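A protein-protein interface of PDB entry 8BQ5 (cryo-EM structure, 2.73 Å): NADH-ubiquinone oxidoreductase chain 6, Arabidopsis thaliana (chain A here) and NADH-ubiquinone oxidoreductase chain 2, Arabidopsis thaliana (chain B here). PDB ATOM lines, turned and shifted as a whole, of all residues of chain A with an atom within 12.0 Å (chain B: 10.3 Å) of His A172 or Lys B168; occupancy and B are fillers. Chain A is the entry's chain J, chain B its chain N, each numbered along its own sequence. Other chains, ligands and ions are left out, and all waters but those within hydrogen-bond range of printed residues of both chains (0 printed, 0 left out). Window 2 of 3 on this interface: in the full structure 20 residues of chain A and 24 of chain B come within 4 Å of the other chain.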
ATOM      1  N   MET A 163       2.031 -10.464  20.638  1.00  0.00           N
ATOM      2  CA  MET A 163       1.158 -10.520  19.463  1.00  0.00           C
ATOM      3  C   MET A 163       1.957 -10.398  18.167  1.00  0.00           C
ATOM      4  O   MET A 163       1.791 -11.201  17.232  1.00  0.00           O
ATOM      5  CB  MET A 163       0.093  -9.422  19.535  1.00  0.00           C
ATOM      6  CG  MET A 163      -0.499  -9.212  20.913  1.00  0.00           C
ATOM      7  SD  MET A 163      -1.562  -7.759  21.038  1.00  0.00           S
ATOM      8  CE  MET A 163      -2.912  -8.232  19.967  1.00  0.00           C
ATOM      9  N   ILE A 164       2.840  -9.398  18.100  1.00  0.00           N
ATOM     10  CA  ILE A 164       3.612  -9.177  16.879  1.00  0.00           C
ATOM     11  C   ILE A 164       4.477 -10.392  16.568  1.00  0.00           C
ATOM     12  O   ILE A 164       4.561 -10.835  15.416  1.00  0.00           O
ATOM     13  CB  ILE A 164       4.462  -7.899  16.996  1.00  0.00           C
ATOM     14  CG1 ILE A 164       3.578  -6.659  16.903  1.00  0.00           C
ATOM     15  CG2 ILE A 164       5.532  -7.872  15.916  1.00  0.00           C
ATOM     16  CD1 ILE A 164       4.269  -5.397  17.342  1.00  0.00           C
ATOM     17  N   GLY A 165       5.150 -10.933  17.586  1.00  0.00           N
ATOM     18  CA  GLY A 165       6.006 -12.084  17.362  1.00  0.00           C
ATOM     19  C   GLY A 165       5.232 -13.296  16.889  1.00  0.00           C
ATOM     20  O   GLY A 165       5.658 -13.996  15.964  1.00  0.00           O
ATOM     21  N   ALA A 166       4.071 -13.547  17.500  1.00  0.00           N
ATOM     22  CA  ALA A 166       3.237 -14.657  17.062  1.00  0.00           C
ATOM     23  C   ALA A 166       2.891 -14.530  15.587  1.00  0.00           C
ATOM     24  O   ALA A 166       2.953 -15.514  14.843  1.00  0.00           O
ATOM     25  CB  ALA A 166       1.966 -14.727  17.906  1.00  0.00           C
ATOM     26  N   ILE A 167       2.542 -13.322  15.139  1.00  0.00           N
ATOM     27  CA  ILE A 167       2.202 -13.163  13.726  1.00  0.00           C
ATOM     28  C   ILE A 167       3.430 -13.348  12.841  1.00  0.00           C
ATOM     29  O   ILE A 167       3.410 -14.132  11.887  1.00  0.00           O
ATOM     30  CB  ILE A 167       1.535 -11.805  13.470  1.00  0.00           C
ATOM     31  CG1 ILE A 167       0.119 -11.823  14.009  1.00  0.00           C
ATOM     32  CG2 ILE A 167       1.526 -11.495  11.982  1.00  0.00           C
ATOM     33  CD1 ILE A 167      -0.667 -13.066  13.679  1.00  0.00           C
ATOM     34  N   VAL A 168       4.518 -12.636  13.143  1.00  0.00           N
ATOM     35  CA  VAL A 168       5.646 -12.633  12.216  1.00  0.00           C
ATOM     36  C   VAL A 168       6.271 -14.015  12.116  1.00  0.00           C
ATOM     37  O   VAL A 168       6.846 -14.366  11.079  1.00  0.00           O
ATOM     38  CB  VAL A 168       6.699 -11.575  12.606  1.00  0.00           C
ATOM     39  CG1 VAL A 168       6.086 -10.192  12.615  1.00  0.00           C
ATOM     40  CG2 VAL A 168       7.334 -11.902  13.942  1.00  0.00           C
ATOM     41  N   LEU A 169       6.163 -14.831  13.164  1.00  0.00           N
ATOM     42  CA  LEU A 169       6.838 -16.120  13.118  1.00  0.00           C
ATOM     43  C   LEU A 169       5.992 -17.215  12.471  1.00  0.00           C
ATOM     44  O   LEU A 169       6.544 -18.089  11.800  1.00  0.00           O
ATOM     45  CB  LEU A 169       7.270 -16.528  14.526  1.00  0.00           C
ATOM     46  CG  LEU A 169       8.341 -15.598  15.113  1.00  0.00           C
ATOM     47  CD1 LEU A 169       8.347 -15.608  16.633  1.00  0.00           C
ATOM     48  CD2 LEU A 169       9.716 -15.944  14.571  1.00  0.00           C
ATOM     49  N   THR A 170       4.666 -17.189  12.628  1.00  0.00           N
ATOM     50  CA  THR A 170       3.849 -18.320  12.206  1.00  0.00           C
ATOM     51  C   THR A 170       2.885 -18.044  11.060  1.00  0.00           C
ATOM     52  O   THR A 170       2.368 -19.006  10.484  1.00  0.00           O
ATOM     53  CB  THR A 170       3.033 -18.867  13.390  1.00  0.00           C
ATOM     54  OG1 THR A 170       2.127 -17.862  13.858  1.00  0.00           O
ATOM     55  CG2 THR A 170       3.953 -19.288  14.523  1.00  0.00           C
ATOM     56  N   MET A 171       2.629 -16.787  10.710  1.00  0.00           N
ATOM     57  CA  MET A 171       1.558 -16.475   9.769  1.00  0.00           C
ATOM     58  C   MET A 171       1.911 -16.908   8.350  1.00  0.00           C
ATOM     59  O   MET A 171       2.962 -16.542   7.818  1.00  0.00           O
ATOM     60  CB  MET A 171       1.260 -14.976   9.798  1.00  0.00           C
ATOM     61  CG  MET A 171       0.168 -14.515   8.844  1.00  0.00           C
ATOM     62  SD  MET A 171      -1.194 -15.680   8.658  1.00  0.00           S
ATOM     63  CE  MET A 171      -2.354 -15.013   9.843  1.00  0.00           C
ATOM     64  N   HIS A 172       1.015 -17.681   7.737  1.00  0.00           N
ATOM     65  CA  HIS A 172       1.060 -18.006   6.311  1.00  0.00           C
ATOM     66  C   HIS A 172      -0.316 -17.677   5.742  1.00  0.00           C
ATOM     67  O   HIS A 172      -1.214 -18.523   5.767  1.00  0.00           O
ATOM     68  CB  HIS A 172       1.404 -19.471   6.067  1.00  0.00           C
ATOM     69  CG  HIS A 172       2.863 -19.782   6.167  1.00  0.00           C
ATOM     70  ND1 HIS A 172       3.493 -20.016   7.369  1.00  0.00           N
ATOM     71  CD2 HIS A 172       3.813 -19.913   5.212  1.00  0.00           C
ATOM     72  CE1 HIS A 172       4.770 -20.269   7.151  1.00  0.00           C
ATOM     73  NE2 HIS A 172       4.990 -20.213   5.849  1.00  0.00           N
ATOM     74  N   ARG A 173      -0.486 -16.462   5.233  1.00  0.00           N
ATOM     75  CA  ARG A 173      -1.795 -16.041   4.751  1.00  0.00           C
ATOM     76  C   ARG A 173      -2.176 -16.804   3.489  1.00  0.00           C
ATOM     77  O   ARG A 173      -1.320 -17.139   2.666  1.00  0.00           O
ATOM     78  CB  ARG A 173      -1.812 -14.538   4.489  1.00  0.00           C
ATOM     79  CG  ARG A 173      -3.211 -13.950   4.400  1.00  0.00           C
ATOM     80  CD  ARG A 173      -3.165 -12.438   4.314  1.00  0.00           C
ATOM     81  NE  ARG A 173      -4.480 -11.838   4.499  1.00  0.00           N
ATOM     82  CZ  ARG A 173      -4.683 -10.582   4.871  1.00  0.00           C
ATOM     83  NH1 ARG A 173      -3.674  -9.761   5.111  1.00  0.00           N
ATOM     84  NH2 ARG A 173      -5.929 -10.139   5.008  1.00  0.00           N
ATOM     85  N   THR A 174      -3.469 -17.073   3.341  1.00  0.00           N
ATOM     86  CA  THR A 174      -3.988 -17.814   2.199  1.00  0.00           C
ATOM     87  C   THR A 174      -4.359 -16.889   1.044  1.00  0.00           C
ATOM     88  O   THR A 174      -4.092 -17.195  -0.116  1.00  0.00           O
ATOM     89  CB  THR A 174      -5.220 -18.643   2.590  1.00  0.00           C
ATOM     90  OG1 THR A 174      -6.318 -17.765   2.864  1.00  0.00           O
ATOM     91  CG2 THR A 174      -4.928 -19.484   3.820  1.00  0.00           C
ATOM     92  N   PHE B 120      15.376  -9.089   3.027  1.00  0.00           N
ATOM     93  CA  PHE B 120      14.627  -9.201   4.272  1.00  0.00           C
ATOM     94  C   PHE B 120      13.621  -8.055   4.274  1.00  0.00           C
ATOM     95  O   PHE B 120      13.972  -6.911   4.568  1.00  0.00           O
ATOM     96  CB  PHE B 120      15.580  -9.133   5.459  1.00  0.00           C
ATOM     97  CG  PHE B 120      14.958  -9.492   6.770  1.00  0.00           C
ATOM     98  CD1 PHE B 120      14.232  -8.552   7.482  1.00  0.00           C
ATOM     99  CD2 PHE B 120      15.126 -10.753   7.309  1.00  0.00           C
ATOM    100  CE1 PHE B 120      13.670  -8.871   8.697  1.00  0.00           C
ATOM    101  CE2 PHE B 120      14.568 -11.078   8.525  1.00  0.00           C
ATOM    102  CZ  PHE B 120      13.837 -10.136   9.221  1.00  0.00           C
ATOM    103  N   VAL B 161      12.208 -13.049  19.665  1.00  0.00           N
ATOM    104  CA  VAL B 161      11.495 -12.980  18.395  1.00  0.00           C
ATOM    105  C   VAL B 161      12.453 -12.663  17.249  1.00  0.00           C
ATOM    106  O   VAL B 161      12.398 -13.299  16.189  1.00  0.00           O
ATOM    107  CB  VAL B 161      10.339 -11.969  18.469  1.00  0.00           C
ATOM    108  CG1 VAL B 161       9.704 -11.804  17.101  1.00  0.00           C
ATOM    109  CG2 VAL B 161       9.307 -12.430  19.484  1.00  0.00           C
ATOM    110  N   ALA B 163      15.647 -13.148  16.985  1.00  0.00           N
ATOM    111  CA  ALA B 163      16.663 -14.163  16.731  1.00  0.00           C
ATOM    112  C   ALA B 163      16.137 -15.270  15.826  1.00  0.00           C
ATOM    113  O   ALA B 163      16.920 -15.938  15.143  1.00  0.00           O
ATOM    114  CB  ALA B 163      17.171 -14.745  18.049  1.00  0.00           C
ATOM    115  N   ALA B 164      14.821 -15.479  15.805  1.00  0.00           N
ATOM    116  CA  ALA B 164      14.194 -16.451  14.922  1.00  0.00           C
ATOM    117  C   ALA B 164      13.538 -15.794  13.712  1.00  0.00           C
ATOM    118  O   ALA B 164      12.579 -16.342  13.159  1.00  0.00           O
ATOM    119  CB  ALA B 164      13.172 -17.283  15.695  1.00  0.00           C
ATOM    120  N   SER B 165      14.046 -14.634  13.286  1.00  0.00           N
ATOM    121  CA  SER B 165      13.384 -13.859  12.240  1.00  0.00           C
ATOM    122  C   SER B 165      13.463 -14.550  10.882  1.00  0.00           C
ATOM    123  O   SER B 165      12.550 -14.413  10.060  1.00  0.00           O
ATOM    124  CB  SER B 165      13.983 -12.456  12.167  1.00  0.00           C
ATOM    125  OG  SER B 165      15.378 -12.482  12.407  1.00  0.00           O
ATOM    126  N   LYS B 166      14.547 -15.273  10.615  1.00  0.00           N
ATOM    127  CA  LYS B 166      14.634 -16.083   9.400  1.00  0.00           C
ATOM    128  C   LYS B 166      13.930 -17.399   9.696  1.00  0.00           C
ATOM    129  O   LYS B 166      14.559 -18.425   9.949  1.00  0.00           O
ATOM    130  CB  LYS B 166      16.082 -16.304   8.980  1.00  0.00           C
ATOM    131  CG  LYS B 166      16.830 -15.037   8.616  1.00  0.00           C
ATOM    132  CD  LYS B 166      17.361 -15.092   7.193  1.00  0.00           C
ATOM    133  CE  LYS B 166      16.219 -15.080   6.188  1.00  0.00           C
ATOM    134  NZ  LYS B 166      16.692 -15.040   4.777  1.00  0.00           N
ATOM    135  N   ARG B 167      12.599 -17.362   9.669  1.00  0.00           N
ATOM    136  CA  ARG B 167      11.798 -18.452  10.207  1.00  0.00           C
ATOM    137  C   ARG B 167      11.889 -19.735   9.391  1.00  0.00           C
ATOM    138  O   ARG B 167      11.506 -20.793   9.898  1.00  0.00           O
ATOM    139  CB  ARG B 167      10.336 -18.017  10.326  1.00  0.00           C
ATOM    140  CG  ARG B 167       9.615 -17.891   9.006  1.00  0.00           C
ATOM    141  CD  ARG B 167       8.421 -16.966   9.107  1.00  0.00           C
ATOM    142  NE  ARG B 167       7.611 -17.015   7.898  1.00  0.00           N
ATOM    143  CZ  ARG B 167       6.323 -16.706   7.845  1.00  0.00           C
ATOM    144  NH1 ARG B 167       5.662 -16.308   8.919  1.00  0.00           N
ATOM    145  NH2 ARG B 167       5.683 -16.799   6.683  1.00  0.00           N
ATOM    146  N   LYS B 168      12.381 -19.680   8.156  1.00  0.00           N
ATOM    147  CA  LYS B 168      12.539 -20.873   7.338  1.00  0.00           C
ATOM    148  C   LYS B 168      13.923 -21.496   7.457  1.00  0.00           C
ATOM    149  O   LYS B 168      14.150 -22.576   6.905  1.00  0.00           O
ATOM    150  CB  LYS B 168      12.246 -20.550   5.870  1.00  0.00           C
ATOM    151  CG  LYS B 168      10.772 -20.409   5.572  1.00  0.00           C
ATOM    152  CD  LYS B 168       9.982 -21.499   6.265  1.00  0.00           C
ATOM    153  CE  LYS B 168       8.535 -21.492   5.826  1.00  0.00           C
ATOM    154  NZ  LYS B 168       7.802 -20.386   6.492  1.00  0.00           N
ATOM    155  N   SER B 169      14.840 -20.854   8.169  1.00  0.00           N
ATOM    156  CA  SER B 169      16.207 -21.336   8.280  1.00  0.00           C
ATOM    157  C   SER B 169      16.342 -22.267   9.477  1.00  0.00           C
ATOM    158  O   SER B 169      15.789 -22.006  10.548  1.00  0.00           O
ATOM    159  CB  SER B 169      17.174 -20.158   8.411  1.00  0.00           C
ATOM    160  OG  SER B 169      18.346 -20.518   9.119  1.00  0.00           O
ATOM    161  N   GLU B 170      17.070 -23.368   9.280  1.00  0.00           N
ATOM    162  CA  GLU B 170      17.351 -24.276  10.388  1.00  0.00           C
ATOM    163  C   GLU B 170      18.153 -23.579  11.476  1.00  0.00           C
ATOM    164  O   GLU B 170      17.861 -23.725  12.668  1.00  0.00           O
ATOM    165  CB  GLU B 170      18.108 -25.507   9.884  1.00  0.00           C
ATOM    166  CG  GLU B 170      17.386 -26.314   8.818  1.00  0.00           C
ATOM    167  CD  GLU B 170      17.494 -25.714   7.424  1.00  0.00           C
ATOM    168  OE1 GLU B 170      17.749 -24.498   7.302  1.00  0.00           O
ATOM    169  OE2 GLU B 170      17.309 -26.464   6.444  1.00  0.00           O
ATOM    170  N   PHE B 171      19.164 -22.806  11.079  1.00  0.00           N
ATOM    171  CA  PHE B 171      20.029 -22.151  12.050  1.00  0.00           C
ATOM    172  C   PHE B 171      19.265 -21.114  12.866  1.00  0.00           C
ATOM    173  O   PHE B 171      19.396 -21.054  14.092  1.00  0.00           O
ATOM    174  CB  PHE B 171      21.216 -21.516  11.330  1.00  0.00           C
ATOM    175  CG  PHE B 171      22.046 -22.496  10.552  1.00  0.00           C
ATOM    176  CD1 PHE B 171      22.820 -23.439  11.205  1.00  0.00           C
ATOM    177  CD2 PHE B 171      22.049 -22.480   9.167  1.00  0.00           C
ATOM    178  CE1 PHE B 171      23.588 -24.343  10.495  1.00  0.00           C
ATOM    179  CE2 PHE B 171      22.814 -23.382   8.450  1.00  0.00           C
ATOM    180  CZ  PHE B 171      23.583 -24.315   9.117  1.00  0.00           C
ATOM    181  N   SER B 172      18.455 -20.288  12.200  1.00  0.00           N
ATOM    182  CA  SER B 172      17.744 -19.226  12.906  1.00  0.00           C
ATOM    183  C   SER B 172      16.692 -19.795  13.855  1.00  0.00           C
ATOM    184  O   SER B 172      16.558 -19.327  14.992  1.00  0.00           O
ATOM    185  CB  SER B 172      17.114 -18.264  11.900  1.00  0.00           C
ATOM    186  OG  SER B 172      16.521 -17.153  12.547  1.00  0.00           O
ATOM    187  N   THR B 173      15.946 -20.811  13.415  1.00  0.00           N
ATOM    188  CA  THR B 173      14.968 -21.443  14.298  1.00  0.00           C
ATOM    189  C   THR B 173      15.647 -22.128  15.479  1.00  0.00           C
ATOM    190  O   THR B 173      15.161 -22.051  16.614  1.00  0.00           O
ATOM    191  CB  THR B 173      14.120 -22.448  13.518  1.00  0.00           C
ATOM    192  OG1 THR B 173      14.977 -23.360  12.823  1.00  0.00           O
ATOM    193  CG2 THR B 173      13.228 -21.734  12.518  1.00  0.00           C
ATOM    194  N   GLU B 174      16.771 -22.808  15.233  1.00  0.00           N
ATOM    195  CA  GLU B 174      17.499 -23.451  16.322  1.00  0.00           C
ATOM    196  C   GLU B 174      17.990 -22.425  17.336  1.00  0.00           C
ATOM    197  O   GLU B 174      17.881 -22.631  18.553  1.00  0.00           O
ATOM    198  CB  GLU B 174      18.672 -24.257  15.763  1.00  0.00           C
ATOM    199  CG  GLU B 174      19.361 -25.142  16.787  1.00  0.00           C
ATOM    200  CD  GLU B 174      20.561 -25.879  16.218  1.00  0.00           C
ATOM    201  OE1 GLU B 174      20.448 -26.443  15.111  1.00  0.00           O
ATOM    202  OE2 GLU B 174      21.619 -25.895  16.882  1.00  0.00           O
ATOM    203  N   GLY B 256      23.741 -18.368  14.996  1.00  0.00           N
ATOM    204  CA  GLY B 256      22.523 -18.737  14.292  1.00  0.00           C
ATOM    205  C   GLY B 256      21.604 -17.590  13.928  1.00  0.00           C
ATOM    206  O   GLY B 256      20.846 -17.708  12.961  1.00  0.00           O
ATOM    207  N   PRO B 258      20.386 -13.871  12.471  1.00  0.00           N
ATOM    208  CA  PRO B 258      20.848 -13.037  11.354  1.00  0.00           C
ATOM    209  C   PRO B 258      21.886 -12.036  11.832  1.00  0.00           C
ATOM    210  O   PRO B 258      21.830 -11.551  12.963  1.00  0.00           O
ATOM    211  CB  PRO B 258      19.568 -12.349  10.861  1.00  0.00           C
ATOM    212  CG  PRO B 258      18.442 -13.116  11.487  1.00  0.00           C
ATOM    213  CD  PRO B 258      18.972 -13.609  12.785  1.00  0.00           C
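The backbone carbonyl oxygen (O) of Ala A166 is in hydrogen-bond range of the side-chain hydroxyl (OG1) of Thr A170. ND1 of His A172 is in hydrogen-bond range of O of Thr A170, at 3.5 Å. The side-chain sulfur of Met A171 is in hydrogen-bond range of the backbone NH of Arg A173 (3.6 Å).
Of the 12 printed residues of chain A, 6 touch a printed residue of chain B. Hydrophobic or aromatic side chains of chain A that line the printed part of chain B: Val A168, Leu A169 and His A172. Of the 16 printed residues of chain B, 4 touch a printed residue of chain A. Printed residues of chain B that touch a printed residue of chain A: Val B161, Ala B164, Arg B167 and Lys B168. Hydrophobic or aromatic side chains of chain B within 4 Å of the printed part of chain A: Val B161 and Ala B164. Among the printed residues, 9 pairs touch across the chains.
CA of Gly A165 touches CG1 of Val B161, at 3.7 Å. Val A168 touches Val B161. CD2 of Leu A169 touches O of Ala B164, 3.2 Å away. Thr A170 touches Arg B167 (C to NH1, 3.9 Å). Arg B167 touches His A172 (NH2 to NE2, 3.6 Å).
Of the printed residues of chain B, His A172 touches Arg B167 and Lys B168. Of chain A, only His A172 (2.9 Å) comes within 4 Å of Lys B168. Ser B169 touches none of the printed residues of chain A. No residue of chain A comes within 4 Å of Glu B170. Printed residues of chain B within 4 Å of Gly A165: Val B161. Of the printed residues of chain B, Val A168 touches Val B161 (3.95 Å) and Arg B167 (3.1 Å). Ile A167 touches none of the printed residues of chain B. Ser B172 touches none of the printed residues of chain A. The nearest residue of chain B that does not touch His A172 is Lys B166 (9.9 Å). The nearest printed residue of chain B that does not touch Gly A165 is Arg B167 (7.4 Å).
NH1 of Arg B167 is in hydrogen-bond range of O of Val A168. O of Leu A169 sits close to NH1 of Arg B167 (3.5 Å). The guanidinium group (NH1) of Arg B167 sits at hydrogen-bond distance from the backbone carbonyl oxygen (O) of Met A171 (2.9 Å). A ring nitrogen (NE2) of His A172 is in hydrogen-bond range of the side-chain amino group (NZ) of Lys B168.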
